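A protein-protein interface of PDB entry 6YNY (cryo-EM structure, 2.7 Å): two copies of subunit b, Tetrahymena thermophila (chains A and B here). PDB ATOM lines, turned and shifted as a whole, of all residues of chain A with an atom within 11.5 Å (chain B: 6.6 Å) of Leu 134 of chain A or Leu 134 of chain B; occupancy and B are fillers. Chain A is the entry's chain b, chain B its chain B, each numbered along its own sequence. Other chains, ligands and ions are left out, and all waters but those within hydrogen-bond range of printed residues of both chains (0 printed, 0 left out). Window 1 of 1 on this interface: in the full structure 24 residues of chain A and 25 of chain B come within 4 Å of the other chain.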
ATOM      1  N   GLY A 121     -30.387  -7.928  37.361  1.00  0.00           N
ATOM      2  CA  GLY A 121     -30.616  -8.022  35.934  1.00  0.00           C
ATOM      3  C   GLY A 121     -30.245  -6.771  35.175  1.00  0.00           C
ATOM      4  O   GLY A 121     -29.982  -6.845  33.972  1.00  0.00           O
ATOM      5  N   PHE A 123     -27.475  -4.951  35.804  1.00  0.00           N
ATOM      6  CA  PHE A 123     -26.045  -5.065  35.556  1.00  0.00           C
ATOM      7  C   PHE A 123     -25.712  -6.260  34.676  1.00  0.00           C
ATOM      8  O   PHE A 123     -24.687  -6.248  33.987  1.00  0.00           O
ATOM      9  CB  PHE A 123     -25.292  -5.142  36.881  1.00  0.00           C
ATOM     10  CG  PHE A 123     -25.231  -3.838  37.609  1.00  0.00           C
ATOM     11  CD1 PHE A 123     -24.488  -2.788  37.108  1.00  0.00           C
ATOM     12  CD2 PHE A 123     -25.919  -3.658  38.791  1.00  0.00           C
ATOM     13  CE1 PHE A 123     -24.433  -1.586  37.769  1.00  0.00           C
ATOM     14  CE2 PHE A 123     -25.867  -2.455  39.460  1.00  0.00           C
ATOM     15  CZ  PHE A 123     -25.122  -1.418  38.947  1.00  0.00           C
ATOM     16  N   VAL A 124     -26.551  -7.295  34.685  1.00  0.00           N
ATOM     17  CA  VAL A 124     -26.393  -8.378  33.722  1.00  0.00           C
ATOM     18  C   VAL A 124     -26.653  -7.867  32.312  1.00  0.00           C
ATOM     19  O   VAL A 124     -25.882  -8.131  31.383  1.00  0.00           O
ATOM     20  CB  VAL A 124     -27.322  -9.551  34.076  1.00  0.00           C
ATOM     21  CG1 VAL A 124     -27.366 -10.551  32.944  1.00  0.00           C
ATOM     22  CG2 VAL A 124     -26.860 -10.221  35.341  1.00  0.00           C
ATOM     23  N   LEU A 125     -27.746  -7.125  32.135  1.00  0.00           N
ATOM     24  CA  LEU A 125     -28.018  -6.502  30.846  1.00  0.00           C
ATOM     25  C   LEU A 125     -26.963  -5.460  30.512  1.00  0.00           C
ATOM     26  O   LEU A 125     -26.536  -5.349  29.357  1.00  0.00           O
ATOM     27  CB  LEU A 125     -29.408  -5.877  30.853  1.00  0.00           C
ATOM     28  CG  LEU A 125     -30.577  -6.853  30.921  1.00  0.00           C
ATOM     29  CD1 LEU A 125     -31.861  -6.111  31.158  1.00  0.00           C
ATOM     30  CD2 LEU A 125     -30.674  -7.654  29.650  1.00  0.00           C
ATOM     31  N   ASN A 126     -26.531  -4.688  31.508  1.00  0.00           N
ATOM     32  CA  ASN A 126     -25.463  -3.720  31.293  1.00  0.00           C
ATOM     33  C   ASN A 126     -24.240  -4.394  30.690  1.00  0.00           C
ATOM     34  O   ASN A 126     -23.709  -3.955  29.664  1.00  0.00           O
ATOM     35  CB  ASN A 126     -25.110  -3.048  32.618  1.00  0.00           C
ATOM     36  CG  ASN A 126     -24.211  -1.854  32.446  1.00  0.00           C
ATOM     37  OD1 ASN A 126     -23.064  -1.978  32.020  1.00  0.00           O
ATOM     38  ND2 ASN A 126     -24.721  -0.684  32.801  1.00  0.00           N
ATOM     39  N   PHE A 127     -23.782  -5.477  31.320  1.00  0.00           N
ATOM     40  CA  PHE A 127     -22.645  -6.223  30.798  1.00  0.00           C
ATOM     41  C   PHE A 127     -22.972  -6.860  29.454  1.00  0.00           C
ATOM     42  O   PHE A 127     -22.129  -6.883  28.551  1.00  0.00           O
ATOM     43  CB  PHE A 127     -22.224  -7.284  31.811  1.00  0.00           C
ATOM     44  CG  PHE A 127     -21.033  -8.085  31.394  1.00  0.00           C
ATOM     45  CD1 PHE A 127     -19.756  -7.663  31.707  1.00  0.00           C
ATOM     46  CD2 PHE A 127     -21.190  -9.267  30.695  1.00  0.00           C
ATOM     47  CE1 PHE A 127     -18.661  -8.400  31.325  1.00  0.00           C
ATOM     48  CE2 PHE A 127     -20.100 -10.005  30.312  1.00  0.00           C
ATOM     49  CZ  PHE A 127     -18.832  -9.572  30.627  1.00  0.00           C
ATOM     50  N   GLY A 128     -24.189  -7.381  29.300  1.00  0.00           N
ATOM     51  CA  GLY A 128     -24.570  -7.986  28.037  1.00  0.00           C
ATOM     52  C   GLY A 128     -24.712  -6.972  26.918  1.00  0.00           C
ATOM     53  O   GLY A 128     -24.326  -7.235  25.777  1.00  0.00           O
ATOM     54  N   MET A 129     -25.279  -5.806  27.225  1.00  0.00           N
ATOM     55  CA  MET A 129     -25.364  -4.740  26.237  1.00  0.00           C
ATOM     56  C   MET A 129     -23.996  -4.138  25.954  1.00  0.00           C
ATOM     57  O   MET A 129     -23.751  -3.647  24.848  1.00  0.00           O
ATOM     58  CB  MET A 129     -26.329  -3.664  26.722  1.00  0.00           C
ATOM     59  CG  MET A 129     -27.748  -4.152  26.908  1.00  0.00           C
ATOM     60  SD  MET A 129     -28.769  -2.994  27.825  1.00  0.00           S
ATOM     61  CE  MET A 129     -28.764  -1.612  26.698  1.00  0.00           C
ATOM     62  N   ALA A 130     -23.100  -4.170  26.938  1.00  0.00           N
ATOM     63  CA  ALA A 130     -21.744  -3.675  26.751  1.00  0.00           C
ATOM     64  C   ALA A 130     -20.876  -4.683  26.013  1.00  0.00           C
ATOM     65  O   ALA A 130     -20.016  -4.299  25.214  1.00  0.00           O
ATOM     66  CB  ALA A 130     -21.126  -3.345  28.105  1.00  0.00           C
ATOM     67  N   THR A 131     -21.086  -5.969  26.271  1.00  0.00           N
ATOM     68  CA  THR A 131     -20.267  -7.037  25.706  1.00  0.00           C
ATOM     69  C   THR A 131     -20.903  -7.499  24.403  1.00  0.00           C
ATOM     70  O   THR A 131     -21.894  -8.231  24.403  1.00  0.00           O
ATOM     71  CB  THR A 131     -20.139  -8.178  26.707  1.00  0.00           C
ATOM     72  OG1 THR A 131     -19.667  -7.658  27.953  1.00  0.00           O
ATOM     73  CG2 THR A 131     -19.177  -9.222  26.213  1.00  0.00           C
ATOM     74  N   VAL A 132     -20.315  -7.079  23.286  1.00  0.00           N
ATOM     75  CA  VAL A 132     -20.890  -7.380  21.983  1.00  0.00           C
ATOM     76  C   VAL A 132     -20.513  -8.773  21.489  1.00  0.00           C
ATOM     77  O   VAL A 132     -21.292  -9.404  20.767  1.00  0.00           O
ATOM     78  CB  VAL A 132     -20.460  -6.304  20.976  1.00  0.00           C
ATOM     79  CG1 VAL A 132     -21.048  -6.592  19.622  1.00  0.00           C
ATOM     80  CG2 VAL A 132     -20.879  -4.932  21.457  1.00  0.00           C
ATOM     81  N   ASP A 133     -19.340  -9.281  21.855  1.00  0.00           N
ATOM     82  CA  ASP A 133     -18.888 -10.601  21.432  1.00  0.00           C
ATOM     83  C   ASP A 133     -18.960 -11.614  22.571  1.00  0.00           C
ATOM     84  O   ASP A 133     -18.071 -12.447  22.744  1.00  0.00           O
ATOM     85  CB  ASP A 133     -17.477 -10.525  20.861  1.00  0.00           C
ATOM     86  CG  ASP A 133     -17.243 -11.531  19.748  1.00  0.00           C
ATOM     87  OD1 ASP A 133     -18.134 -12.372  19.498  1.00  0.00           O
ATOM     88  OD2 ASP A 133     -16.173 -11.473  19.108  1.00  0.00           O
ATOM     89  N   LEU A 134     -20.021 -11.532  23.375  1.00  0.00           N
ATOM     90  CA  LEU A 134     -20.186 -12.453  24.492  1.00  0.00           C
ATOM     91  C   LEU A 134     -20.147 -13.907  24.036  1.00  0.00           C
ATOM     92  O   LEU A 134     -19.747 -14.787  24.805  1.00  0.00           O
ATOM     93  CB  LEU A 134     -21.497 -12.148  25.212  1.00  0.00           C
ATOM     94  CG  LEU A 134     -21.838 -12.933  26.474  1.00  0.00           C
ATOM     95  CD1 LEU A 134     -20.686 -12.936  27.447  1.00  0.00           C
ATOM     96  CD2 LEU A 134     -23.055 -12.323  27.114  1.00  0.00           C
ATOM     97  N   ASN A 135     -20.554 -14.177  22.795  1.00  0.00           N
ATOM     98  CA  ASN A 135     -20.457 -15.530  22.260  1.00  0.00           C
ATOM     99  C   ASN A 135     -19.008 -15.978  22.132  1.00  0.00           C
ATOM    100  O   ASN A 135     -18.692 -17.154  22.340  1.00  0.00           O
ATOM    101  CB  ASN A 135     -21.157 -15.600  20.905  1.00  0.00           C
ATOM    102  CG  ASN A 135     -21.004 -16.944  20.238  1.00  0.00           C
ATOM    103  OD1 ASN A 135     -20.151 -17.126  19.375  1.00  0.00           O
ATOM    104  ND2 ASN A 135     -21.830 -17.893  20.634  1.00  0.00           N
ATOM    105  N   TRP A 136     -18.111 -15.055  21.785  1.00  0.00           N
ATOM    106  CA  TRP A 136     -16.696 -15.386  21.699  1.00  0.00           C
ATOM    107  C   TRP A 136     -16.116 -15.724  23.064  1.00  0.00           C
ATOM    108  O   TRP A 136     -15.178 -16.521  23.158  1.00  0.00           O
ATOM    109  CB  TRP A 136     -15.938 -14.222  21.071  1.00  0.00           C
ATOM    110  CG  TRP A 136     -14.477 -14.429  20.926  1.00  0.00           C
ATOM    111  CD1 TRP A 136     -13.848 -15.140  19.956  1.00  0.00           C
ATOM    112  CD2 TRP A 136     -13.448 -13.904  21.768  1.00  0.00           C
ATOM    113  NE1 TRP A 136     -12.494 -15.098  20.140  1.00  0.00           N
ATOM    114  CE2 TRP A 136     -12.222 -14.344  21.249  1.00  0.00           C
ATOM    115  CE3 TRP A 136     -13.447 -13.106  22.913  1.00  0.00           C
ATOM    116  CZ2 TRP A 136     -11.008 -14.016  21.835  1.00  0.00           C
ATOM    117  CZ3 TRP A 136     -12.243 -12.784  23.489  1.00  0.00           C
ATOM    118  CH2 TRP A 136     -11.040 -13.237  22.951  1.00  0.00           C
ATOM    119  N   ILE A 137     -16.663 -15.137  24.124  1.00  0.00           N
ATOM    120  CA  ILE A 137     -16.175 -15.415  25.467  1.00  0.00           C
ATOM    121  C   ILE A 137     -16.684 -16.762  25.952  1.00  0.00           C
ATOM    122  O   ILE A 137     -15.959 -17.513  26.610  1.00  0.00           O
ATOM    123  CB  ILE A 137     -16.584 -14.273  26.412  1.00  0.00           C
ATOM    124  CG1 ILE A 137     -16.062 -12.944  25.875  1.00  0.00           C
ATOM    125  CG2 ILE A 137     -16.062 -14.519  27.807  1.00  0.00           C
ATOM    126  CD1 ILE A 137     -16.400 -11.764  26.719  1.00  0.00           C
ATOM    127  N   MET A 138     -17.939 -17.086  25.641  1.00  0.00           N
ATOM    128  CA  MET A 138     -18.486 -18.384  26.011  1.00  0.00           C
ATOM    129  C   MET A 138     -17.702 -19.514  25.359  1.00  0.00           C
ATOM    130  O   MET A 138     -17.285 -20.465  26.027  1.00  0.00           O
ATOM    131  CB  MET A 138     -19.956 -18.454  25.612  1.00  0.00           C
ATOM    132  CG  MET A 138     -20.870 -17.565  26.420  1.00  0.00           C
ATOM    133  SD  MET A 138     -21.483 -18.376  27.899  1.00  0.00           S
ATOM    134  CE  MET A 138     -22.726 -17.203  28.405  1.00  0.00           C
ATOM    135  N   LYS A 139     -17.493 -19.424  24.045  1.00  0.00           N
ATOM    136  CA  LYS A 139     -16.761 -20.466  23.338  1.00  0.00           C
ATOM    137  C   LYS A 139     -15.318 -20.550  23.809  1.00  0.00           C
ATOM    138  O   LYS A 139     -14.741 -21.641  23.873  1.00  0.00           O
ATOM    139  CB  LYS A 139     -16.823 -20.209  21.837  1.00  0.00           C
ATOM    140  CG  LYS A 139     -18.197 -20.369  21.255  1.00  0.00           C
ATOM    141  CD  LYS A 139     -18.231 -20.000  19.796  1.00  0.00           C
ATOM    142  CE  LYS A 139     -19.514 -20.451  19.150  1.00  0.00           C
ATOM    143  NZ  LYS A 139     -19.539 -20.143  17.715  1.00  0.00           N
ATOM    144  N   SER A 140     -14.713 -19.411  24.138  1.00  0.00           N
ATOM    145  CA  SER A 140     -13.347 -19.407  24.637  1.00  0.00           C
ATOM    146  C   SER A 140     -13.250 -19.916  26.067  1.00  0.00           C
ATOM    147  O   SER A 140     -12.136 -20.098  26.569  1.00  0.00           O
ATOM    148  CB  SER A 140     -12.767 -17.998  24.534  1.00  0.00           C
ATOM    149  OG  SER A 140     -12.767 -17.547  23.198  1.00  0.00           O
ATOM    150  N   THR A 141     -14.381 -20.154  26.726  1.00  0.00           N
ATOM    151  CA  THR A 141     -14.418 -20.670  28.084  1.00  0.00           C
ATOM    152  C   THR A 141     -14.778 -22.147  28.151  1.00  0.00           C
ATOM    153  O   THR A 141     -14.667 -22.746  29.224  1.00  0.00           O
ATOM    154  CB  THR A 141     -15.423 -19.864  28.918  1.00  0.00           C
ATOM    155  OG1 THR A 141     -15.131 -18.469  28.810  1.00  0.00           O
ATOM    156  CG2 THR A 141     -15.368 -20.266  30.369  1.00  0.00           C
ATOM    157  N   TYR A 142     -15.190 -22.750  27.037  1.00  0.00           N
ATOM    158  CA  TYR A 142     -15.650 -24.133  27.068  1.00  0.00           C
ATOM    159  C   TYR A 142     -14.541 -25.082  27.502  1.00  0.00           C
ATOM    160  O   TYR A 142     -14.725 -25.893  28.415  1.00  0.00           O
ATOM    161  CB  TYR A 142     -16.191 -24.531  25.698  1.00  0.00           C
ATOM    162  CG  TYR A 142     -16.645 -25.965  25.624  1.00  0.00           C
ATOM    163  CD1 TYR A 142     -17.881 -26.342  26.116  1.00  0.00           C
ATOM    164  CD2 TYR A 142     -15.840 -26.941  25.062  1.00  0.00           C
ATOM    165  CE1 TYR A 142     -18.301 -27.646  26.053  1.00  0.00           C
ATOM    166  CE2 TYR A 142     -16.252 -28.246  24.995  1.00  0.00           C
ATOM    167  CZ  TYR A 142     -17.484 -28.596  25.491  1.00  0.00           C
ATOM    168  OH  TYR A 142     -17.897 -29.902  25.424  1.00  0.00           O
ATOM    169  N   PHE B 127     -25.952 -22.753  25.812  1.00  0.00           N
ATOM    170  CA  PHE B 127     -26.831 -21.714  25.293  1.00  0.00           C
ATOM    171  C   PHE B 127     -26.033 -20.534  24.753  1.00  0.00           C
ATOM    172  O   PHE B 127     -26.387 -19.961  23.717  1.00  0.00           O
ATOM    173  CB  PHE B 127     -27.791 -21.260  26.389  1.00  0.00           C
ATOM    174  CG  PHE B 127     -28.732 -20.189  25.958  1.00  0.00           C
ATOM    175  CD1 PHE B 127     -29.912 -20.511  25.316  1.00  0.00           C
ATOM    176  CD2 PHE B 127     -28.442 -18.859  26.192  1.00  0.00           C
ATOM    177  CE1 PHE B 127     -30.781 -19.530  24.913  1.00  0.00           C
ATOM    178  CE2 PHE B 127     -29.308 -17.874  25.792  1.00  0.00           C
ATOM    179  CZ  PHE B 127     -30.480 -18.209  25.151  1.00  0.00           C
ATOM    180  N   GLY B 128     -24.952 -20.159  25.437  1.00  0.00           N
ATOM    181  CA  GLY B 128     -24.142 -19.045  24.972  1.00  0.00           C
ATOM    182  C   GLY B 128     -23.366 -19.377  23.715  1.00  0.00           C
ATOM    183  O   GLY B 128     -23.288 -18.567  22.788  1.00  0.00           O
ATOM    184  N   THR B 131     -26.171 -19.436  21.114  1.00  0.00           N
ATOM    185  CA  THR B 131     -26.787 -18.141  20.830  1.00  0.00           C
ATOM    186  C   THR B 131     -25.695 -17.167  20.409  1.00  0.00           C
ATOM    187  O   THR B 131     -24.952 -16.647  21.243  1.00  0.00           O
ATOM    188  CB  THR B 131     -27.547 -17.641  22.052  1.00  0.00           C
ATOM    189  OG1 THR B 131     -28.544 -18.597  22.423  1.00  0.00           O
ATOM    190  CG2 THR B 131     -28.206 -16.314  21.764  1.00  0.00           C
ATOM    191  N   VAL B 132     -25.608 -16.912  19.107  1.00  0.00           N
ATOM    192  CA  VAL B 132     -24.583 -16.023  18.578  1.00  0.00           C
ATOM    193  C   VAL B 132     -24.998 -14.555  18.624  1.00  0.00           C
ATOM    194  O   VAL B 132     -24.136 -13.673  18.667  1.00  0.00           O
ATOM    195  CB  VAL B 132     -24.227 -16.436  17.144  1.00  0.00           C
ATOM    196  CG1 VAL B 132     -23.106 -15.571  16.609  1.00  0.00           C
ATOM    197  CG2 VAL B 132     -23.841 -17.892  17.096  1.00  0.00           C
ATOM    198  N   ASP B 133     -26.298 -14.269  18.618  1.00  0.00           N
ATOM    199  CA  ASP B 133     -26.805 -12.901  18.664  1.00  0.00           C
ATOM    200  C   ASP B 133     -27.288 -12.537  20.059  1.00  0.00           C
ATOM    201  O   ASP B 133     -28.282 -11.830  20.231  1.00  0.00           O
ATOM    202  CB  ASP B 133     -27.923 -12.724  17.643  1.00  0.00           C
ATOM    203  CG  ASP B 133     -27.915 -11.356  16.992  1.00  0.00           C
ATOM    204  OD1 ASP B 133     -27.043 -10.526  17.327  1.00  0.00           O
ATOM    205  OD2 ASP B 133     -28.787 -11.116  16.135  1.00  0.00           O
ATOM    206  N   LEU B 134     -26.583 -13.026  21.076  1.00  0.00           N
ATOM    207  CA  LEU B 134     -26.998 -12.812  22.454  1.00  0.00           C
ATOM    208  C   LEU B 134     -27.004 -11.335  22.825  1.00  0.00           C
ATOM    209  O   LEU B 134     -27.830 -10.905  23.636  1.00  0.00           O
ATOM    210  CB  LEU B 134     -26.079 -13.605  23.377  1.00  0.00           C
ATOM    211  CG  LEU B 134     -26.368 -13.655  24.870  1.00  0.00           C
ATOM    212  CD1 LEU B 134     -27.794 -14.065  25.154  1.00  0.00           C
ATOM    213  CD2 LEU B 134     -25.408 -14.631  25.490  1.00  0.00           C
ATOM    214  N   ASN B 135     -26.096 -10.546  22.250  1.00  0.00           N
ATOM    215  CA  ASN B 135     -26.112  -9.109  22.499  1.00  0.00           C
ATOM    216  C   ASN B 135     -27.400  -8.477  21.992  1.00  0.00           C
ATOM    217  O   ASN B 135     -27.931  -7.548  22.609  1.00  0.00           O
ATOM    218  CB  ASN B 135     -24.900  -8.454  21.845  1.00  0.00           C
ATOM    219  CG  ASN B 135     -24.868  -6.959  22.043  1.00  0.00           C
ATOM    220  OD1 ASN B 135     -25.191  -6.194  21.139  1.00  0.00           O
ATOM    221  ND2 ASN B 135     -24.482  -6.532  23.235  1.00  0.00           N
ATOM    222  N   TRP B 136     -27.920  -8.973  20.871  1.00  0.00           N
ATOM    223  CA  TRP B 136     -29.192  -8.486  20.358  1.00  0.00           C
ATOM    224  C   TRP B 136     -30.342  -8.841  21.289  1.00  0.00           C
ATOM    225  O   TRP B 136     -31.335  -8.109  21.352  1.00  0.00           O
ATOM    226  CB  TRP B 136     -29.424  -9.061  18.967  1.00  0.00           C
ATOM    227  CG  TRP B 136     -30.722  -8.702  18.347  1.00  0.00           C
ATOM    228  CD1 TRP B 136     -31.021  -7.561  17.673  1.00  0.00           C
ATOM    229  CD2 TRP B 136     -31.904  -9.502  18.323  1.00  0.00           C
ATOM    230  NE1 TRP B 136     -32.317  -7.595  17.237  1.00  0.00           N
ATOM    231  CE2 TRP B 136     -32.882  -8.779  17.624  1.00  0.00           C
ATOM    232  CE3 TRP B 136     -32.229 -10.759  18.829  1.00  0.00           C
ATOM    233  CZ2 TRP B 136     -34.162  -9.271  17.421  1.00  0.00           C
ATOM    234  CZ3 TRP B 136     -33.497 -11.242  18.625  1.00  0.00           C
ATOM    235  CH2 TRP B 136     -34.448 -10.502  17.928  1.00  0.00           C
ATOM    236  N   ILE B 137     -30.223  -9.947  22.021  1.00  0.00           N
ATOM    237  CA  ILE B 137     -31.258 -10.331  22.972  1.00  0.00           C
ATOM    238  C   ILE B 137     -31.175  -9.484  24.235  1.00  0.00           C
ATOM    239  O   ILE B 137     -32.200  -9.064  24.779  1.00  0.00           O
ATOM    240  CB  ILE B 137     -31.144 -11.832  23.283  1.00  0.00           C
ATOM    241  CG1 ILE B 137     -31.518 -12.643  22.045  1.00  0.00           C
ATOM    242  CG2 ILE B 137     -32.021 -12.209  24.456  1.00  0.00           C
ATOM    243  CD1 ILE B 137     -31.318 -14.111  22.188  1.00  0.00           C
ATOM    244  N   MET B 138     -29.962  -9.228  24.726  1.00  0.00           N
ATOM    245  CA  MET B 138     -29.808  -8.405  25.919  1.00  0.00           C
ATOM    246  C   MET B 138     -30.311  -6.988  25.675  1.00  0.00           C
ATOM    247  O   MET B 138     -31.026  -6.418  26.505  1.00  0.00           O
ATOM    248  CB  MET B 138     -28.345  -8.386  26.353  1.00  0.00           C
ATOM    249  CG  MET B 138     -27.797  -9.718  26.814  1.00  0.00           C
ATOM    250  SD  MET B 138     -28.427 -10.244  28.412  1.00  0.00           S
ATOM    251  CE  MET B 138     -27.228 -11.506  28.814  1.00  0.00           C
ATOM    252  N   LYS B 139     -29.939  -6.401  24.537  1.00  0.00           N
ATOM    253  CA  LYS B 139     -30.410  -5.061  24.207  1.00  0.00           C
ATOM    254  C   LYS B 139     -31.913  -5.040  23.972  1.00  0.00           C
ATOM    255  O   LYS B 139     -32.590  -4.078  24.345  1.00  0.00           O
ATOM    256  CB  LYS B 139     -29.666  -4.539  22.980  1.00  0.00           C
ATOM    257  CG  LYS B 139     -28.233  -4.160  23.247  1.00  0.00           C
ATOM    258  CD  LYS B 139     -27.493  -3.808  21.982  1.00  0.00           C
ATOM    259  CE  LYS B 139     -26.127  -3.249  22.300  1.00  0.00           C
ATOM    260  NZ  LYS B 139     -25.372  -2.879  21.090  1.00  0.00           N
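Leu 125 of chain A touches Met 138 of chain B (CD2 to O, 3.4 Å). CA of Gly 128 of chain A touches CG of Met 138 of chain B, at 3.9 Å. Lys 139 of chain B touches Met 129 of chain A (CE to O, 3.5 Å). Asn 135 of chain B touches Val 132 of chain A. CD2 of Leu 134 of chain B touches CD2 of Leu 134 of chain A, at 3.7 Å. Asn 135 of chain A touches Val 132 of chain B. Met 138 of chain A touches Gly 128 of chain B.
Of the 11 printed residues of chain B, 7 touch a printed residue of chain A. Hydrophobic or aromatic side chains of chain B within 4 Å of the printed part of chain A: Leu 134 and Met 138. Of the 21 printed residues of chain A, 8 touch a printed residue of chain B. Printed residues of chain A that touch a printed residue of chain B: Leu 125, Gly 128, Met 129, Thr 131, Val 132, Leu 134, Asn 135 and Met 138. Hydrophobic or aromatic side chains of chain A that line the printed part of chain B: Leu 125, Met 129, Leu 134 and Met 138. Among the printed residues, 12 pairs touch across the chains. Among the printed residues, no Asp or Glu carboxylate lies within 4 Å of a Lys or Arg side-chain nitrogen of the other chain.
Gly 128 of chain A touches Met 138 of chain B, and with the chains exchanged Met 138 of chain A touches Gly 128 of chain B. Thr 131 of chain A touches Asn 135 of chain B, and with the chains exchanged Asn 135 of chain A touches Thr 131 of chain B. Val 132 of chain A touches Asn 135 of chain B, and with the chains exchanged Asn 135 of chain A touches Val 132 of chain B. Leu 134 of chain A touches its own counterpart, Leu 134 of chain B. Positions printed for both chains: 127, 128, 131, 132, 133, 134, 135, 136, 137, 138 and 139.
O of Thr 131 of chain B sits at hydrogen-bond distance from ND2 of Asn 135 of chain A, at 3.4 Å. ND2 of Asn 135 of chain B sits at hydrogen-bond distance from O of Met 129 of chain A, at 3.4 Å. The backbone carbonyl oxygen of Thr 131 of chain A is in hydrogen-bond range of the side-chain amide nitrogen of Asn 135 of chain B (3.3 Å). The side-chain amide nitrogen (ND2) of Asn 135 of chain A sits at hydrogen-bond distance from the backbone carbonyl oxygen (O) of Gly 128 of chain B (2.7 Å). O of Gly 128 of chain A sits at hydrogen-bond distance from ND2 of Asn 135 of chain B, at 2.6 Å.
Leu 134 of chain A touches just one residue of chain B: Leu 134 (3.7 Å). No residue of chain A comes within 4 Å of Ile 137 of chain B. Of the printed residues of chain B, Asn 135 of chain A touches Gly 128, Thr 131 and Val 132. Of the printed residues of chain B, Leu 125 of chain A touches Met 138 (3.4 Å). Printed residues of chain A within 4 Å of Met 138 of chain B: Leu 125 (3.4 Å) and Gly 128 (3.9 Å). Of the printed residues of chain B, Met 129 of chain A touches Asn 135 (3.4 Å) and Lys 139 (3.5 Å). The nearest residue of chain A that does not touch Leu 134 of chain B is Met 138 of chain A (4.7 Å).
O of Phe 127 of chain B is in hydrogen-bond range of OG1 of Thr 131 of chain B (2.9 Å). OD1 of Asn 135 of chain B sits close to NZ of Lys 139 of chain B, at 3.3 Å. The side-chain hydroxyl (OG1) of Thr 131 of chain A sits at hydrogen-bond distance from the backbone carbonyl oxygen (O) of Phe 127 of chain A (2.6 Å). NZ of Lys 139 of chain A lies close to OD1 of Asn 135 of chain A, 3.5 Å away.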
